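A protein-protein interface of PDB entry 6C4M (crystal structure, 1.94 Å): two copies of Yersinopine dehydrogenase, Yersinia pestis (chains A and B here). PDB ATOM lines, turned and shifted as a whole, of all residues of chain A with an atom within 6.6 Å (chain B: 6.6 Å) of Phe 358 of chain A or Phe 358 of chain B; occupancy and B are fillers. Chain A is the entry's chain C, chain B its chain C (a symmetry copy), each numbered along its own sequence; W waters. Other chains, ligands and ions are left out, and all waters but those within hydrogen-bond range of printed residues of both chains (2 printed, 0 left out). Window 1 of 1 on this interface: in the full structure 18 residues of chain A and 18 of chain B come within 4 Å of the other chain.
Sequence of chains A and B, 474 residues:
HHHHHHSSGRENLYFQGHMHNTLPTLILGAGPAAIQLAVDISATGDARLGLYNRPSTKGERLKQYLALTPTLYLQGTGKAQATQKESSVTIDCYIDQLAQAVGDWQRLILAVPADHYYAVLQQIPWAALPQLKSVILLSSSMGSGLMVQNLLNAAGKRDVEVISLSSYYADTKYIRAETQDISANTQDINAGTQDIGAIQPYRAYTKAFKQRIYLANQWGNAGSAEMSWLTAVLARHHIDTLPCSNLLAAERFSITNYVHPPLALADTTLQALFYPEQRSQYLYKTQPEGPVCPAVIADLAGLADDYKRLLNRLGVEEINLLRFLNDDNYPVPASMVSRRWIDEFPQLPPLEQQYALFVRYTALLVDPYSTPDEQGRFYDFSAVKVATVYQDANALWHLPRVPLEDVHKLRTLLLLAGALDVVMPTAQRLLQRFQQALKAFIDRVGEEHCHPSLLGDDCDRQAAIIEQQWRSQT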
ATOM      1  N   THR A 286      18.920   2.380  33.204  1.00  0.00           N
ATOM      2  CA  THR A 286      20.180   1.647  33.137  1.00  0.00           C
ATOM      3  C   THR A 286      20.337   0.712  34.337  1.00  0.00           C
ATOM      4  O   THR A 286      19.747   0.903  35.404  1.00  0.00           O
ATOM      5  CB  THR A 286      21.401   2.577  33.105  1.00  0.00           C
ATOM      6  OG1 THR A 286      21.581   3.158  34.396  1.00  0.00           O
ATOM      7  CG2 THR A 286      21.283   3.679  32.099  1.00  0.00           C
ATOM      8  N   VAL A 292      18.930  -1.326  30.618  1.00  0.00           N
ATOM      9  CA  VAL A 292      19.813  -0.701  29.638  1.00  0.00           C
ATOM     10  C   VAL A 292      21.270  -0.856  30.044  1.00  0.00           C
ATOM     11  O   VAL A 292      21.695  -0.442  31.125  1.00  0.00           O
ATOM     12  CB  VAL A 292      19.437   0.774  29.428  1.00  0.00           C
ATOM     13  CG1 VAL A 292      20.402   1.408  28.461  1.00  0.00           C
ATOM     14  CG2 VAL A 292      18.016   0.836  28.862  1.00  0.00           C
ATOM     15  N   CYS A 293      22.047  -1.394  29.135  1.00  0.00           N
ATOM     16  CA  CYS A 293      23.448  -1.676  29.342  1.00  0.00           C
ATOM     17  C   CYS A 293      23.995  -2.086  27.982  1.00  0.00           C
ATOM     18  O   CYS A 293      23.214  -2.389  27.080  1.00  0.00           O
ATOM     19  CB  CYS A 293      23.626  -2.802  30.368  1.00  0.00           C
ATOM     20  SG  CYS A 293      22.999  -4.413  29.835  1.00  0.00           S
ATOM     21  N   PRO A 294      25.309  -2.175  27.809  1.00  0.00           N
ATOM     22  CA  PRO A 294      25.834  -2.521  26.478  1.00  0.00           C
ATOM     23  C   PRO A 294      25.295  -3.828  25.882  1.00  0.00           C
ATOM     24  O   PRO A 294      25.029  -3.850  24.677  1.00  0.00           O
ATOM     25  CB  PRO A 294      27.347  -2.562  26.731  1.00  0.00           C
ATOM     26  CG  PRO A 294      27.548  -1.525  27.808  1.00  0.00           C
ATOM     27  CD  PRO A 294      26.386  -1.742  28.725  1.00  0.00           C
ATOM     28  N   ILE A 297      21.811  -3.161  24.556  1.00  0.00           N
ATOM     29  CA  ILE A 297      21.880  -2.320  23.364  1.00  0.00           C
ATOM     30  C   ILE A 297      22.387  -3.122  22.173  1.00  0.00           C
ATOM     31  O   ILE A 297      21.939  -2.925  21.033  1.00  0.00           O
ATOM     32  CB  ILE A 297      22.768  -1.089  23.655  1.00  0.00           C
ATOM     33  CG1 ILE A 297      22.040  -0.153  24.633  1.00  0.00           C
ATOM     34  CG2 ILE A 297      23.202  -0.384  22.388  1.00  0.00           C
ATOM     35  CD1 ILE A 297      20.743   0.434  24.071  1.00  0.00           C
ATOM     36  N   MET A 336      24.017  15.123  22.332  1.00  0.00           N
ATOM     37  CA  MET A 336      24.073  13.711  22.681  1.00  0.00           C
ATOM     38  C   MET A 336      24.142  12.847  21.425  1.00  0.00           C
ATOM     39  O   MET A 336      25.136  12.161  21.194  1.00  0.00           O
ATOM     40  CB  MET A 336      22.864  13.350  23.544  1.00  0.00           C
ATOM     41  CG  MET A 336      22.810  14.136  24.826  1.00  0.00           C
ATOM     42  SD  MET A 336      24.258  13.707  25.931  1.00  0.00           S
ATOM     43  CE  MET A 336      23.670  12.168  26.561  1.00  0.00           C
ATOM     44  N   GLN A 353      27.078   2.015  15.975  1.00  0.00           N
ATOM     45  CA  GLN A 353      25.635   1.928  16.116  1.00  0.00           C
ATOM     46  C   GLN A 353      25.242   1.750  17.570  1.00  0.00           C
ATOM     47  O   GLN A 353      24.338   2.432  18.080  1.00  0.00           O
ATOM     48  CB  GLN A 353      25.091   0.751  15.282  1.00  0.00           C
ATOM     49  CG  GLN A 353      25.026   0.991  13.777  1.00  0.00           C
ATOM     50  CD  GLN A 353      24.193  -0.101  13.086  1.00  0.00           C
ATOM     51  OE1 GLN A 353      23.837  -1.116  13.697  1.00  0.00           O
ATOM     52  NE2 GLN A 353      23.869   0.115  11.831  1.00  0.00           N
ATOM     53  N   GLN A 354      25.927   0.835  18.263  1.00  0.00           N
ATOM     54  CA  GLN A 354      25.571   0.559  19.636  1.00  0.00           C
ATOM     55  C   GLN A 354      25.829   1.764  20.522  1.00  0.00           C
ATOM     56  O   GLN A 354      24.971   2.148  21.327  1.00  0.00           O
ATOM     57  CB  GLN A 354      26.342  -0.674  20.115  1.00  0.00           C
ATOM     58  CG  GLN A 354      25.759  -1.994  19.517  1.00  0.00           C
ATOM     59  CD  GLN A 354      26.664  -3.185  19.792  1.00  0.00           C
ATOM     60  OE1 GLN A 354      27.263  -3.273  20.847  1.00  0.00           O
ATOM     61  NE2 GLN A 354      26.809  -4.061  18.819  1.00  0.00           N
ATOM     62  N   TYR A 355      27.018   2.361  20.407  1.00  0.00           N
ATOM     63  CA  TYR A 355      27.324   3.559  21.187  1.00  0.00           C
ATOM     64  C   TYR A 355      26.231   4.600  20.975  1.00  0.00           C
ATOM     65  O   TYR A 355      25.663   5.128  21.942  1.00  0.00           O
ATOM     66  CB  TYR A 355      28.718   4.090  20.797  1.00  0.00           C
ATOM     67  CG  TYR A 355      29.273   5.287  21.582  1.00  0.00           C
ATOM     68  CD1 TYR A 355      28.731   5.681  22.793  1.00  0.00           C
ATOM     69  CD2 TYR A 355      30.353   6.004  21.091  1.00  0.00           C
ATOM     70  CE1 TYR A 355      29.235   6.749  23.477  1.00  0.00           C
ATOM     71  CE2 TYR A 355      30.866   7.097  21.769  1.00  0.00           C
ATOM     72  CZ  TYR A 355      30.306   7.463  22.964  1.00  0.00           C
ATOM     73  OH  TYR A 355      30.831   8.516  23.676  1.00  0.00           O
ATOM     74  N   ALA A 356      25.856   4.835  19.707  1.00  0.00           N
ATOM     75  CA  ALA A 356      24.828   5.833  19.420  1.00  0.00           C
ATOM     76  C   ALA A 356      23.516   5.493  20.110  1.00  0.00           C
ATOM     77  O   ALA A 356      22.874   6.377  20.693  1.00  0.00           O
ATOM     78  CB  ALA A 356      24.626   5.981  17.916  1.00  0.00           C
ATOM     79  N   LEU A 357      23.122   4.207  20.101  1.00  0.00           N
ATOM     80  CA  LEU A 357      21.875   3.820  20.743  1.00  0.00           C
ATOM     81  C   LEU A 357      21.947   3.921  22.254  1.00  0.00           C
ATOM     82  O   LEU A 357      20.955   4.326  22.888  1.00  0.00           O
ATOM     83  CB  LEU A 357      21.484   2.406  20.312  1.00  0.00           C
ATOM     84  CG  LEU A 357      20.972   2.282  18.874  1.00  0.00           C
ATOM     85  CD1 LEU A 357      20.986   0.798  18.428  1.00  0.00           C
ATOM     86  CD2 LEU A 357      19.553   2.878  18.778  1.00  0.00           C
ATOM     87  N   PHE A 358      23.099   3.532  22.864  1.00  0.00           N
ATOM     88  CA  PHE A 358      23.250   3.707  24.303  1.00  0.00           C
ATOM     89  C   PHE A 358      23.151   5.175  24.665  1.00  0.00           C
ATOM     90  O   PHE A 358      22.475   5.543  25.634  1.00  0.00           O
ATOM     91  CB  PHE A 358      24.576   3.097  24.817  1.00  0.00           C
ATOM     92  CG  PHE A 358      24.701   3.169  26.309  1.00  0.00           C
ATOM     93  CD1 PHE A 358      25.155   4.319  26.916  1.00  0.00           C
ATOM     94  CD2 PHE A 358      24.294   2.115  27.103  1.00  0.00           C
ATOM     95  CE1 PHE A 358      25.235   4.409  28.297  1.00  0.00           C
ATOM     96  CE2 PHE A 358      24.387   2.194  28.472  1.00  0.00           C
ATOM     97  CZ  PHE A 358      24.858   3.358  29.065  1.00  0.00           C
ATOM     98  N   VAL A 359      23.765   6.042  23.865  1.00  0.00           N
ATOM     99  CA  VAL A 359      23.679   7.470  24.158  1.00  0.00           C
ATOM    100  C   VAL A 359      22.233   7.924  24.041  1.00  0.00           C
ATOM    101  O   VAL A 359      21.708   8.635  24.915  1.00  0.00           O
ATOM    102  CB  VAL A 359      24.626   8.282  23.244  1.00  0.00           C
ATOM    103  CG1 VAL A 359      24.420   9.766  23.454  1.00  0.00           C
ATOM    104  CG2 VAL A 359      26.080   7.969  23.554  1.00  0.00           C
ATOM    105  N   ARG A 360      21.556   7.491  22.979  1.00  0.00           N
ATOM    106  CA  ARG A 360      20.155   7.852  22.817  1.00  0.00           C
ATOM    107  C   ARG A 360      19.322   7.495  24.047  1.00  0.00           C
ATOM    108  O   ARG A 360      18.623   8.352  24.594  1.00  0.00           O
ATOM    109  CB  ARG A 360      19.595   7.177  21.572  1.00  0.00           C
ATOM    110  CG  ARG A 360      18.320   7.810  21.142  1.00  0.00           C
ATOM    111  CD  ARG A 360      17.222   6.841  21.193  1.00  0.00           C
ATOM    112  NE  ARG A 360      15.974   7.507  20.888  1.00  0.00           N
ATOM    113  CZ  ARG A 360      14.788   7.027  21.180  1.00  0.00           C
ATOM    114  NH1 ARG A 360      14.677   5.824  21.766  1.00  0.00           N
ATOM    115  NH2 ARG A 360      13.719   7.757  20.870  1.00  0.00           N
ATOM    116  N   TYR A 361      19.392   6.233  24.519  1.00  0.00           N
ATOM    117  CA  TYR A 361      18.567   5.854  25.664  1.00  0.00           C
ATOM    118  C   TYR A 361      19.005   6.523  26.959  1.00  0.00           C
ATOM    119  O   TYR A 361      18.169   6.789  27.832  1.00  0.00           O
ATOM    120  CB  TYR A 361      18.514   4.331  25.782  1.00  0.00           C
ATOM    121  CG  TYR A 361      17.495   3.820  24.805  1.00  0.00           C
ATOM    122  CD1 TYR A 361      16.156   3.742  25.157  1.00  0.00           C
ATOM    123  CD2 TYR A 361      17.855   3.469  23.508  1.00  0.00           C
ATOM    124  CE1 TYR A 361      15.190   3.336  24.237  1.00  0.00           C
ATOM    125  CE2 TYR A 361      16.899   3.065  22.580  1.00  0.00           C
ATOM    126  CZ  TYR A 361      15.570   3.000  22.943  1.00  0.00           C
ATOM    127  OH  TYR A 361      14.632   2.562  22.012  1.00  0.00           O
ATOM    128  N   THR A 362      20.289   6.812  27.122  1.00  0.00           N
ATOM    129  CA  THR A 362      20.704   7.621  28.268  1.00  0.00           C
ATOM    130  C   THR A 362      20.062   9.003  28.198  1.00  0.00           C
ATOM    131  O   THR A 362      19.467   9.479  29.172  1.00  0.00           O
ATOM    132  CB  THR A 362      22.231   7.704  28.302  1.00  0.00           C
ATOM    133  OG1 THR A 362      22.761   6.393  28.377  1.00  0.00           O
ATOM    134  CG2 THR A 362      22.768   8.573  29.486  1.00  0.00           C
ATOM    135  N   ALA A 363      20.143   9.646  27.031  1.00  0.00           N
ATOM    136  CA  ALA A 363      19.600  10.999  26.881  1.00  0.00           C
ATOM    137  C   ALA A 363      18.097  11.032  27.140  1.00  0.00           C
ATOM    138  O   ALA A 363      17.574  12.006  27.697  1.00  0.00           O
ATOM    139  CB  ALA A 363      19.889  11.515  25.483  1.00  0.00           C
ATOM    140  N   THR B 286      24.800  14.332  32.358  1.00  0.00           N
ATOM    141  CA  THR B 286      24.723  14.376  30.902  1.00  0.00           C
ATOM    142  C   THR B 286      24.003  15.639  30.426  1.00  0.00           C
ATOM    143  O   THR B 286      23.209  16.255  31.143  1.00  0.00           O
ATOM    144  CB  THR B 286      23.983  13.166  30.315  1.00  0.00           C
ATOM    145  OG1 THR B 286      22.587  13.293  30.589  1.00  0.00           O
ATOM    146  CG2 THR B 286      24.457  11.856  30.862  1.00  0.00           C
ATOM    147  N   VAL B 292      28.459  15.899  30.218  1.00  0.00           N
ATOM    148  CA  VAL B 292      28.763  14.582  29.669  1.00  0.00           C
ATOM    149  C   VAL B 292      27.990  14.339  28.383  1.00  0.00           C
ATOM    150  O   VAL B 292      26.759  14.395  28.339  1.00  0.00           O
ATOM    151  CB  VAL B 292      28.496  13.482  30.708  1.00  0.00           C
ATOM    152  CG1 VAL B 292      28.759  12.132  30.093  1.00  0.00           C
ATOM    153  CG2 VAL B 292      29.432  13.703  31.899  1.00  0.00           C
ATOM    154  N   CYS B 293      28.721  13.997  27.349  1.00  0.00           N
ATOM    155  CA  CYS B 293      28.186  13.774  26.026  1.00  0.00           C
ATOM    156  C   CYS B 293      29.331  13.197  25.206  1.00  0.00           C
ATOM    157  O   CYS B 293      30.484  13.283  25.629  1.00  0.00           O
ATOM    158  CB  CYS B 293      27.684  15.089  25.418  1.00  0.00           C
ATOM    159  SG  CYS B 293      28.976  16.312  25.094  1.00  0.00           S
ATOM    160  N   PRO B 294      29.077  12.669  24.014  1.00  0.00           N
ATOM    161  CA  PRO B 294      30.179  12.066  23.248  1.00  0.00           C
ATOM    162  C   PRO B 294      31.378  12.987  22.993  1.00  0.00           C
ATOM    163  O   PRO B 294      32.511  12.504  23.083  1.00  0.00           O
ATOM    164  CB  PRO B 294      29.474  11.636  21.956  1.00  0.00           C
ATOM    165  CG  PRO B 294      28.079  11.294  22.417  1.00  0.00           C
ATOM    166  CD  PRO B 294      27.762  12.374  23.404  1.00  0.00           C
ATOM    167  N   ILE B 297      33.419  13.162  26.179  1.00  0.00           N
ATOM    168  CA  ILE B 297      34.094  11.887  26.413  1.00  0.00           C
ATOM    169  C   ILE B 297      35.259  11.714  25.450  1.00  0.00           C
ATOM    170  O   ILE B 297      36.312  11.165  25.812  1.00  0.00           O
ATOM    171  CB  ILE B 297      33.069  10.736  26.299  1.00  0.00           C
ATOM    172  CG1 ILE B 297      32.108  10.785  27.497  1.00  0.00           C
ATOM    173  CG2 ILE B 297      33.739   9.387  26.144  1.00  0.00           C
ATOM    174  CD1 ILE B 297      32.794  10.554  28.845  1.00  0.00           C
ATOM    175  N   MET B 336      27.486  -2.949  33.205  1.00  0.00           N
ATOM    176  CA  MET B 336      27.716  -1.703  32.487  1.00  0.00           C
ATOM    177  C   MET B 336      29.108  -1.691  31.861  1.00  0.00           C
ATOM    178  O   MET B 336      29.242  -1.663  30.639  1.00  0.00           O
ATOM    179  CB  MET B 336      27.518  -0.523  33.436  1.00  0.00           C
ATOM    180  CG  MET B 336      26.129  -0.467  34.014  1.00  0.00           C
ATOM    181  SD  MET B 336      24.865  -0.145  32.673  1.00  0.00           S
ATOM    182  CE  MET B 336      25.117   1.590  32.473  1.00  0.00           C
ATOM    183  N   GLN B 353      37.022   2.813  23.334  1.00  0.00           N
ATOM    184  CA  GLN B 353      37.416   3.512  24.544  1.00  0.00           C
ATOM    185  C   GLN B 353      36.368   4.531  24.948  1.00  0.00           C
ATOM    186  O   GLN B 353      35.966   4.611  26.120  1.00  0.00           O
ATOM    187  CB  GLN B 353      38.772   4.216  24.334  1.00  0.00           C
ATOM    188  CG  GLN B 353      39.992   3.302  24.349  1.00  0.00           C
ATOM    189  CD  GLN B 353      41.289   4.124  24.444  1.00  0.00           C
ATOM    190  OE1 GLN B 353      41.276   5.354  24.307  1.00  0.00           O
ATOM    191  NE2 GLN B 353      42.390   3.455  24.696  1.00  0.00           N
ATOM    192  N   GLN B 354      35.900   5.319  23.975  1.00  0.00           N
ATOM    193  CA  GLN B 354      34.946   6.359  24.289  1.00  0.00           C
ATOM    194  C   GLN B 354      33.631   5.771  24.764  1.00  0.00           C
ATOM    195  O   GLN B 354      33.076   6.211  25.780  1.00  0.00           O
ATOM    196  CB  GLN B 354      34.757   7.253  23.060  1.00  0.00           C
ATOM    197  CG  GLN B 354      35.978   8.201  22.835  1.00  0.00           C
ATOM    198  CD  GLN B 354      35.904   8.907  21.491  1.00  0.00           C
ATOM    199  OE1 GLN B 354      34.833   9.271  21.045  1.00  0.00           O
ATOM    200  NE2 GLN B 354      37.032   9.041  20.824  1.00  0.00           N
ATOM    201  N   TYR B 355      33.101   4.789  24.030  1.00  0.00           N
ATOM    202  CA  TYR B 355      31.864   4.135  24.450  1.00  0.00           C
ATOM    203  C   TYR B 355      32.005   3.648  25.888  1.00  0.00           C
ATOM    204  O   TYR B 355      31.158   3.945  26.743  1.00  0.00           O
ATOM    205  CB  TYR B 355      31.527   2.986  23.477  1.00  0.00           C
ATOM    206  CG  TYR B 355      30.203   2.238  23.684  1.00  0.00           C
ATOM    207  CD1 TYR B 355      29.190   2.751  24.476  1.00  0.00           C
ATOM    208  CD2 TYR B 355      29.986   1.017  23.063  1.00  0.00           C
ATOM    209  CE1 TYR B 355      28.019   2.072  24.650  1.00  0.00           C
ATOM    210  CE2 TYR B 355      28.808   0.313  23.242  1.00  0.00           C
ATOM    211  CZ  TYR B 355      27.825   0.847  24.034  1.00  0.00           C
ATOM    212  OH  TYR B 355      26.629   0.185  24.186  1.00  0.00           O
ATOM    213  N   ALA B 356      33.128   2.977  26.193  1.00  0.00           N
ATOM    214  CA  ALA B 356      33.329   2.461  27.546  1.00  0.00           C
ATOM    215  C   ALA B 356      33.306   3.579  28.576  1.00  0.00           C
ATOM    216  O   ALA B 356      32.675   3.438  29.632  1.00  0.00           O
ATOM    217  CB  ALA B 356      34.631   1.672  27.632  1.00  0.00           C
ATOM    218  N   LEU B 357      33.944   4.724  28.269  1.00  0.00           N
ATOM    219  CA  LEU B 357      33.960   5.829  29.215  1.00  0.00           C
ATOM    220  C   LEU B 357      32.598   6.479  29.365  1.00  0.00           C
ATOM    221  O   LEU B 357      32.227   6.870  30.486  1.00  0.00           O
ATOM    222  CB  LEU B 357      35.009   6.858  28.796  1.00  0.00           C
ATOM    223  CG  LEU B 357      36.464   6.433  29.020  1.00  0.00           C
ATOM    224  CD1 LEU B 357      37.419   7.352  28.218  1.00  0.00           C
ATOM    225  CD2 LEU B 357      36.787   6.476  30.527  1.00  0.00           C
ATOM    226  N   PHE B 358      31.842   6.638  28.245  1.00  0.00           N
ATOM    227  CA  PHE B 358      30.487   7.165  28.356  1.00  0.00           C
ATOM    228  C   PHE B 358      29.638   6.250  29.215  1.00  0.00           C
ATOM    229  O   PHE B 358      28.888   6.714  30.083  1.00  0.00           O
ATOM    230  CB  PHE B 358      29.841   7.378  26.966  1.00  0.00           C
ATOM    231  CG  PHE B 358      28.490   8.021  27.054  1.00  0.00           C
ATOM    232  CD1 PHE B 358      27.370   7.260  27.304  1.00  0.00           C
ATOM    233  CD2 PHE B 358      28.353   9.393  26.960  1.00  0.00           C
ATOM    234  CE1 PHE B 358      26.122   7.850  27.428  1.00  0.00           C
ATOM    235  CE2 PHE B 358      27.115   9.981  27.065  1.00  0.00           C
ATOM    236  CZ  PHE B 358      25.996   9.194  27.307  1.00  0.00           C
ATOM    237  N   VAL B 359      29.784   4.940  29.036  1.00  0.00           N
ATOM    238  CA  VAL B 359      29.006   4.015  29.856  1.00  0.00           C
ATOM    239  C   VAL B 359      29.411   4.168  31.313  1.00  0.00           C
ATOM    240  O   VAL B 359      28.559   4.260  32.214  1.00  0.00           O
ATOM    241  CB  VAL B 359      29.159   2.562  29.352  1.00  0.00           C
ATOM    242  CG1 VAL B 359      28.471   1.599  30.295  1.00  0.00           C
ATOM    243  CG2 VAL B 359      28.530   2.393  27.980  1.00  0.00           C
ATOM    244  N   ARG B 360      30.718   4.234  31.565  1.00  0.00           N
ATOM    245  CA  ARG B 360      31.184   4.418  32.932  1.00  0.00           C
ATOM    246  C   ARG B 360      30.543   5.634  33.600  1.00  0.00           C
ATOM    247  O   ARG B 360      29.973   5.518  34.687  1.00  0.00           O
ATOM    248  CB  ARG B 360      32.702   4.534  32.942  1.00  0.00           C
ATOM    249  CG  ARG B 360      33.250   4.326  34.309  1.00  0.00           C
ATOM    250  CD  ARG B 360      33.949   5.527  34.772  1.00  0.00           C
ATOM    251  NE  ARG B 360      34.368   5.344  36.145  1.00  0.00           N
ATOM    252  CZ  ARG B 360      34.699   6.324  36.955  1.00  0.00           C
ATOM    253  NH1 ARG B 360      34.700   7.590  36.510  1.00  0.00           N
ATOM    254  NH2 ARG B 360      35.038   6.019  38.205  1.00  0.00           N
ATOM    255  N   TYR B 361      30.605   6.820  32.958  1.00  0.00           N
ATOM    256  CA  TYR B 361      30.044   8.007  33.598  1.00  0.00           C
ATOM    257  C   TYR B 361      28.525   7.968  33.696  1.00  0.00           C
ATOM    258  O   TYR B 361      27.950   8.525  34.640  1.00  0.00           O
ATOM    259  CB  TYR B 361      30.552   9.264  32.894  1.00  0.00           C
ATOM    260  CG  TYR B 361      31.930   9.566  33.409  1.00  0.00           C
ATOM    261  CD1 TYR B 361      32.104  10.324  34.558  1.00  0.00           C
ATOM    262  CD2 TYR B 361      33.060   9.048  32.786  1.00  0.00           C
ATOM    263  CE1 TYR B 361      33.374  10.553  35.086  1.00  0.00           C
ATOM    264  CE2 TYR B 361      34.333   9.267  33.306  1.00  0.00           C
ATOM    265  CZ  TYR B 361      34.489  10.016  34.454  1.00  0.00           C
ATOM    266  OH  TYR B 361      35.772  10.253  34.940  1.00  0.00           O
ATOM    267  N   THR B 362      27.846   7.327  32.755  1.00  0.00           N
ATOM    268  CA  THR B 362      26.408   7.114  32.925  1.00  0.00           C
ATOM    269  C   THR B 362      26.145   6.260  34.162  1.00  0.00           C
ATOM    270  O   THR B 362      25.321   6.610  35.015  1.00  0.00           O
ATOM    271  CB  THR B 362      25.837   6.473  31.659  1.00  0.00           C
ATOM    272  OG1 THR B 362      26.107   7.319  30.555  1.00  0.00           O
ATOM    273  CG2 THR B 362      24.304   6.185  31.759  1.00  0.00           C
ATOM    274  N   ALA B 363      26.870   5.146  34.290  1.00  0.00           N
ATOM    275  CA  ALA B 363      26.653   4.237  35.418  1.00  0.00           C
ATOM    276  C   ALA B 363      26.919   4.925  36.753  1.00  0.00           C
ATOM    277  O   ALA B 363      26.237   4.654  37.750  1.00  0.00           O
ATOM    278  CB  ALA B 363      27.558   3.025  35.279  1.00  0.00           C
HETATM  279  O   HOH W   1      26.717  -2.409  23.076  1.00  0.00           O
HETATM  280  O   HOH W   2      32.764   9.931  22.184  1.00  0.00           O
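O of Val 292 of chain A lies close to SD of Met 336 of chain B (3.5 Å).
The backbone carbonyl oxygen (O) of Val 292 of chain B lies close to the side-chain sulfur (SD) of Met 336 of chain A.
Water W2 lies within hydrogen-bond range of OE1 of Gln 354 of chain B (2.5 Å), O of Pro 294 of chain B (2.7 Å) and OH of Tyr 355 of chain A (2.8 Å).
Water W1 lies within hydrogen-bond range of the side-chain amide oxygen (OE1) of Gln 354 of chain A (2.5 Å), the backbone carbonyl oxygen (O) of Pro 294 of chain A (2.7 Å) and the side-chain hydroxyl (OH) of Tyr 355 of chain B (2.8 Å).
Cys 293 of chain A touches Met 336 of chain B.
Met 336 of chain A touches Pro 294 of chain B.
O of Gln 354 of chain A touches OH of Tyr 355 of chain B, at 3.8 Å.
Tyr 355 of chain A touches Pro 294 of chain B.
OH of Tyr 355 of chain A touches CG2 of Ile 297 of chain B, 3.9 Å away.
Phe 358 of chain A touches Met 336 of chain B.
Phe 358 of chain B touches Val 359 of chain A (CE1 to CG2, 3.9 Å).
Thr 362 of chain A touches Thr 286 of chain B (CG2 to CG2, 3.9 Å).
Thr 362 of chain A touches Phe 358 of chain B.
CG2 of Thr 362 of chain A touches CG2 of Thr 362 of chain B (3.6 Å).
Hydrophobic or aromatic side chains of chain B that line the printed part of chain A: Pro 294, Ile 297, Met 336, Tyr 355, Phe 358 and Val 359.
Hydrophobic or aromatic side chains of chain A that line the printed part of chain B: Pro 294, Ile 297, Met 336, Tyr 355, Phe 358 and Val 359.
Among the printed residues, 27 pairs touch across the chains.
Among the printed residues, no Asp or Glu carboxylate lies within 4 Å of a Lys or Arg side-chain nitrogen of the other chain.
Of the printed residues of chain B, Cys 293 of chain A touches Met 336 (3.7 Å).
Of the printed residues of chain B, Ile 297 of chain A touches Tyr 355.
Phe 358 of chain A touches five residues of chain B.
Printed residues of chain A within 4 Å of Met 336 of chain B: Thr 286, Val 292, Cys 293, Pro 294 and Phe 358.
Gln 353 of chain B touches none of the printed residues of chain A.
Of the printed residues of chain A, Gln 354 of chain B touches Tyr 355.
Of chain A, only Met 336, Tyr 355, Phe 358, Val 359 and Thr 362 come within 4 Å of Phe 358 of chain B.
Ala 363 of chain B touches none of the printed residues of chain A.
The nearest residue of chain A that does not touch Phe 358 of chain B is Ala 363 of chain A (5.9 Å).
The nearest printed residue of chain B that does not touch Tyr 355 of chain A is Cys 293 of chain B (5.1 Å).
Thr 286 of chain A touches Thr 362 of chain B, and with the chains exchanged Thr 362 of chain A touches Thr 286 of chain B.
Cys 293 of chain A touches Met 336 of chain B, and with the chains exchanged Met 336 of chain A touches Cys 293 of chain B.
Ile 297 of chain A touches Tyr 355 of chain B, and with the chains exchanged Tyr 355 of chain A touches Ile 297 of chain B.
Met 336 of chain A touches Phe 358 of chain B, and with the chains exchanged Phe 358 of chain A touches Met 336 of chain B.
The side-chain hydroxyl (OG1) of Thr 362 of chain A is in hydrogen-bond range of the backbone carbonyl oxygen (O) of Phe 358 of chain A (2.9 Å).
The backbone carbonyl oxygen (O) of Phe 358 of chain B sits at hydrogen-bond distance from the side-chain hydroxyl (OG1) of Thr 362 of chain B, 2.9 Å away.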
